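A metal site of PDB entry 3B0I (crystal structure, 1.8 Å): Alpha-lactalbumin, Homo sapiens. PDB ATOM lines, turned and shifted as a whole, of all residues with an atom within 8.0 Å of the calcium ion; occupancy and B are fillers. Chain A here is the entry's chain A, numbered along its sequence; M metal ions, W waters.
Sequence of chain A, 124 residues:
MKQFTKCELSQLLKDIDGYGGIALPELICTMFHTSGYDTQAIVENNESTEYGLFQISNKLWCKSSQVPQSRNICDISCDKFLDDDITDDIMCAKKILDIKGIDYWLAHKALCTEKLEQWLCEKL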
ATOM      1  N   THR A  39       0.256   8.354  26.843  1.00  0.00           N
ATOM      2  CA  THR A  39      -0.103   8.641  25.454  1.00  0.00           C
ATOM      3  C   THR A  39       1.064   8.409  24.477  1.00  0.00           C
ATOM      4  O   THR A  39       0.860   8.196  23.305  1.00  0.00           O
ATOM      5  CB  THR A  39      -0.630  10.089  25.284  1.00  0.00           C
ATOM      6  OG1 THR A  39       0.400  11.039  25.623  1.00  0.00           O
ATOM      7  CG2 THR A  39      -1.843  10.326  26.146  1.00  0.00           C
ATOM      8  N   GLY A  52       0.714   4.248  21.803  1.00  0.00           N
ATOM      9  CA  GLY A  52      -0.208   5.110  22.517  1.00  0.00           C
ATOM     10  C   GLY A  52      -0.936   4.486  23.664  1.00  0.00           C
ATOM     11  O   GLY A  52      -0.681   3.332  24.062  1.00  0.00           O
ATOM     12  N   LEU A  53      -1.877   5.254  24.170  1.00  0.00           N
ATOM     13  CA  LEU A  53      -2.765   4.853  25.241  1.00  0.00           C
ATOM     14  C   LEU A  53      -3.480   3.518  24.967  1.00  0.00           C
ATOM     15  O   LEU A  53      -3.611   2.710  25.890  1.00  0.00           O
ATOM     16  CB  LEU A  53      -3.772   5.981  25.481  1.00  0.00           C
ATOM     17  CG  LEU A  53      -4.874   5.857  26.526  1.00  0.00           C
ATOM     18  CD1 LEU A  53      -4.302   5.677  27.907  1.00  0.00           C
ATOM     19  CD2 LEU A  53      -5.764   7.121  26.471  1.00  0.00           C
ATOM     20  N   ILE A  76      -4.727   6.213   9.001  1.00  0.00           N
ATOM     21  CA  ILE A  76      -4.121   7.225   9.804  1.00  0.00           C
ATOM     22  C   ILE A  76      -2.671   6.799  10.027  1.00  0.00           C
ATOM     23  O   ILE A  76      -2.387   5.609  10.048  1.00  0.00           O
ATOM     24  CB  ILE A  76      -4.868   7.393  11.154  1.00  0.00           C
ATOM     25  CG1 ILE A  76      -4.443   8.683  11.863  1.00  0.00           C
ATOM     26  CG2 ILE A  76      -4.731   6.150  12.058  1.00  0.00           C
ATOM     27  CD1 ILE A  76      -5.278   9.009  13.079  1.00  0.00           C
ATOM     28  N   SER A  77      -1.789   7.770  10.103  1.00  0.00           N
ATOM     29  CA  SER A  77      -0.398   7.501  10.464  1.00  0.00           C
ATOM     30  C   SER A  77      -0.348   7.152  11.938  1.00  0.00           C
ATOM     31  O   SER A  77      -0.995   7.817  12.772  1.00  0.00           O
ATOM     32  CB  SER A  77       0.469   8.712  10.210  1.00  0.00           C
ATOM     33  OG  SER A  77       1.817   8.449  10.675  1.00  0.00           O
ATOM     34  N   CYS A  78       0.430   6.120  12.282  1.00  0.00           N
ATOM     35  CA  CYS A  78       0.651   5.741  13.671  1.00  0.00           C
ATOM     36  C   CYS A  78       1.179   6.856  14.591  1.00  0.00           C
ATOM     37  O   CYS A  78       0.950   6.818  15.797  1.00  0.00           O
ATOM     38  CB  CYS A  78       1.586   4.505  13.737  1.00  0.00           C
ATOM     39  SG  CYS A  78       1.094   3.017  12.796  1.00  0.00           S
ATOM     40  N   ASP A  79       1.867   7.852  14.040  1.00  0.00           N
ATOM     41  CA  ASP A  79       2.366   8.946  14.851  1.00  0.00           C
ATOM     42  C   ASP A  79       1.247   9.676  15.565  1.00  0.00           C
ATOM     43  O   ASP A  79       1.451  10.207  16.642  1.00  0.00           O
ATOM     44  CB  ASP A  79       3.252   9.907  14.046  1.00  0.00           C
ATOM     45  CG  ASP A  79       2.487  10.973  13.293  1.00  0.00           C
ATOM     46  OD1 ASP A  79       2.161  10.755  12.100  1.00  0.00           O
ATOM     47  OD2 ASP A  79       2.294  12.073  13.860  1.00  0.00           O
ATOM     48  N   LYS A  80       0.059   9.663  14.973  1.00  0.00           N
ATOM     49  CA  LYS A  80      -1.079  10.315  15.559  1.00  0.00           C
ATOM     50  C   LYS A  80      -1.415   9.705  16.913  1.00  0.00           C
ATOM     51  O   LYS A  80      -1.926  10.403  17.772  1.00  0.00           O
ATOM     52  CB  LYS A  80      -2.274  10.286  14.589  1.00  0.00           C
ATOM     53  CG  LYS A  80      -2.224  11.341  13.497  1.00  0.00           C
ATOM     54  CD  LYS A  80      -2.441  12.799  13.977  1.00  0.00           C
ATOM     55  CE  LYS A  80      -3.899  13.101  14.418  1.00  0.00           C
ATOM     56  NZ  LYS A  80      -3.990  14.235  15.377  1.00  0.00           N
ATOM     57  N   PHE A  81      -1.051   8.439  17.145  1.00  0.00           N
ATOM     58  CA  PHE A  81      -1.289   7.797  18.423  1.00  0.00           C
ATOM     59  C   PHE A  81      -0.247   8.073  19.504  1.00  0.00           C
ATOM     60  O   PHE A  81      -0.310   7.455  20.574  1.00  0.00           O
ATOM     61  CB  PHE A  81      -1.469   6.295  18.244  1.00  0.00           C
ATOM     62  CG  PHE A  81      -2.514   5.911  17.254  1.00  0.00           C
ATOM     63  CD1 PHE A  81      -3.663   6.674  17.095  1.00  0.00           C
ATOM     64  CD2 PHE A  81      -2.363   4.763  16.496  1.00  0.00           C
ATOM     65  CE1 PHE A  81      -4.630   6.285  16.166  1.00  0.00           C
ATOM     66  CE2 PHE A  81      -3.312   4.363  15.574  1.00  0.00           C
ATOM     67  CZ  PHE A  81      -4.472   5.120  15.421  1.00  0.00           C
ATOM     68  N   LEU A  82       0.699   8.979  19.209  1.00  0.00           N
ATOM     69  CA  LEU A  82       1.666   9.429  20.179  1.00  0.00           C
ATOM     70  C   LEU A  82       1.532  10.911  20.474  1.00  0.00           C
ATOM     71  O   LEU A  82       2.367  11.468  21.147  1.00  0.00           O
ATOM     72  CB  LEU A  82       3.106   9.127  19.687  1.00  0.00           C
ATOM     73  CG  LEU A  82       3.411   7.690  19.362  1.00  0.00           C
ATOM     74  CD1 LEU A  82       4.830   7.588  18.772  1.00  0.00           C
ATOM     75  CD2 LEU A  82       3.299   6.835  20.609  1.00  0.00           C
ATOM     76  N   ASP A  83       0.459  11.577  20.035  1.00  0.00           N
ATOM     77  CA  ASP A  83       0.277  12.979  20.428  1.00  0.00           C
ATOM     78  C   ASP A  83      -0.600  13.141  21.707  1.00  0.00           C
ATOM     79  O   ASP A  83      -1.033  12.162  22.309  1.00  0.00           O
ATOM     80  CB  ASP A  83      -0.163  13.827  19.221  1.00  0.00           C
ATOM     81  CG  ASP A  83      -1.514  13.421  18.674  1.00  0.00           C
ATOM     82  OD1 ASP A  83      -2.298  12.849  19.431  1.00  0.00           O
ATOM     83  OD2 ASP A  83      -1.782  13.697  17.481  1.00  0.00           O
ATOM     84  N   ASP A  84      -0.857  14.365  22.153  1.00  0.00           N
ATOM     85  CA  ASP A  84      -1.524  14.562  23.432  1.00  0.00           C
ATOM     86  C   ASP A  84      -3.058  14.541  23.289  1.00  0.00           C
ATOM     87  O   ASP A  84      -3.789  14.664  24.310  1.00  0.00           O
ATOM     88  CB  ASP A  84      -1.065  15.863  24.100  1.00  0.00           C
ATOM     89  CG  ASP A  84      -1.146  17.070  23.169  1.00  0.00           C
ATOM     90  OD1 ASP A  84      -1.352  16.891  21.943  1.00  0.00           O
ATOM     91  OD2 ASP A  84      -0.983  18.214  23.674  1.00  0.00           O
ATOM     92  N   ASP A  85      -3.547  14.368  22.062  1.00  0.00           N
ATOM     93  CA  ASP A  85      -4.999  14.315  21.793  1.00  0.00           C
ATOM     94  C   ASP A  85      -5.380  12.868  21.550  1.00  0.00           C
ATOM     95  O   ASP A  85      -4.971  12.311  20.534  1.00  0.00           O
ATOM     96  CB  ASP A  85      -5.320  15.138  20.555  1.00  0.00           C
ATOM     97  CG  ASP A  85      -6.787  15.158  20.213  1.00  0.00           C
ATOM     98  OD1 ASP A  85      -7.612  14.778  21.089  1.00  0.00           O
ATOM     99  OD2 ASP A  85      -7.112  15.577  19.064  1.00  0.00           O
ATOM    100  N   ILE A  86      -6.162  12.278  22.441  1.00  0.00           N
ATOM    101  CA  ILE A  86      -6.553  10.854  22.285  1.00  0.00           C
ATOM    102  C   ILE A  86      -7.818  10.633  21.430  1.00  0.00           C
ATOM    103  O   ILE A  86      -8.306   9.516  21.251  1.00  0.00           O
ATOM    104  CB  ILE A  86      -6.662  10.097  23.632  1.00  0.00           C
ATOM    105  CG1 ILE A  86      -7.806  10.608  24.505  1.00  0.00           C
ATOM    106  CG2 ILE A  86      -5.327  10.130  24.440  1.00  0.00           C
ATOM    107  CD1 ILE A  86      -8.084   9.711  25.662  1.00  0.00           C
ATOM    108  N   THR A  87      -8.334  11.717  20.870  1.00  0.00           N
ATOM    109  CA  THR A  87      -9.562  11.653  20.037  1.00  0.00           C
ATOM    110  C   THR A  87      -9.414  10.679  18.874  1.00  0.00           C
ATOM    111  O   THR A  87     -10.277   9.835  18.639  1.00  0.00           O
ATOM    112  CB  THR A  87      -9.903  13.036  19.511  1.00  0.00           C
ATOM    113  OG1 THR A  87     -10.061  13.932  20.596  1.00  0.00           O
ATOM    114  CG2 THR A  87     -11.213  13.023  18.670  1.00  0.00           C
ATOM    115  N   ASP A  88      -8.313  10.806  18.113  1.00  0.00           N
ATOM    116  CA  ASP A  88      -8.057   9.881  17.002  1.00  0.00           C
ATOM    117  C   ASP A  88      -7.772   8.461  17.488  1.00  0.00           C
ATOM    118  O   ASP A  88      -8.111   7.492  16.817  1.00  0.00           O
ATOM    119  CB  ASP A  88      -6.895  10.392  16.176  1.00  0.00           C
ATOM    120  CG  ASP A  88      -5.638  10.503  16.993  1.00  0.00           C
ATOM    121  OD1 ASP A  88      -4.774   9.620  16.864  1.00  0.00           O
ATOM    122  OD2 ASP A  88      -5.530  11.411  17.831  1.00  0.00           O
ATOM    123  N   ASP A  89      -7.161   8.336  18.662  1.00  0.00           N
ATOM    124  CA  ASP A  89      -6.881   7.017  19.247  1.00  0.00           C
ATOM    125  C   ASP A  89      -8.191   6.308  19.588  1.00  0.00           C
ATOM    126  O   ASP A  89      -8.361   5.129  19.321  1.00  0.00           O
ATOM    127  CB  ASP A  89      -6.068   7.142  20.531  1.00  0.00           C
ATOM    128  CG  ASP A  89      -4.728   7.877  20.322  1.00  0.00           C
ATOM    129  OD1 ASP A  89      -4.724   9.048  19.869  1.00  0.00           O
ATOM    130  OD2 ASP A  89      -3.689   7.277  20.644  1.00  0.00           O
ATOM    131  N   ILE A  90      -9.089   7.058  20.209  1.00  0.00           N
ATOM    132  CA  ILE A  90     -10.436   6.584  20.502  1.00  0.00           C
ATOM    133  C   ILE A  90     -11.190   6.168  19.206  1.00  0.00           C
ATOM    134  O   ILE A  90     -11.789   5.086  19.179  1.00  0.00           O
ATOM    135  CB  ILE A  90     -11.238   7.626  21.301  1.00  0.00           C
ATOM    136  CG1 ILE A  90     -10.664   7.855  22.694  1.00  0.00           C
ATOM    137  CG2 ILE A  90     -12.679   7.118  21.501  1.00  0.00           C
ATOM    138  CD1 ILE A  90     -11.230   9.105  23.359  1.00  0.00           C
HETATM  139 CA    CA M   1      -3.698  10.939  19.202  1.00  0.00          CA
HETATM  140  O   HOH W   1      -2.363  10.342  21.004  1.00  0.00           O
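The side-chain carboxylate (OD1) of Asp 85 lies within hydrogen-bond range of the side-chain hydroxyl (OG1) of Thr 87, at 2.6 Å.
Five residues have an atom within 4 Å of the calcium ion: Lys 80, Asp 83, Asp 85, Asp 88 and Asp 89.
Water W1 bridges O of Asp 83 and OD2 of Asp 89.
OD1 of Asp 89 is bound to the calcium ion (2.3 Å).
The calcium ion is bound by O of Asp 85, at 2.3 Å.
Water W1 binds the calcium ion, 2.3 Å away.
OD2 of Asp 88 binds the calcium ion.
The calcium ion is bound by the backbone carbonyl oxygen (O) of Lys 80.
The calcium ion is bound by OD1 of Asp 83.
The calcium ion is bound by OD1 of Asp 88 (2.9 Å).
The calcium ion has seven donor atoms within binding distance.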
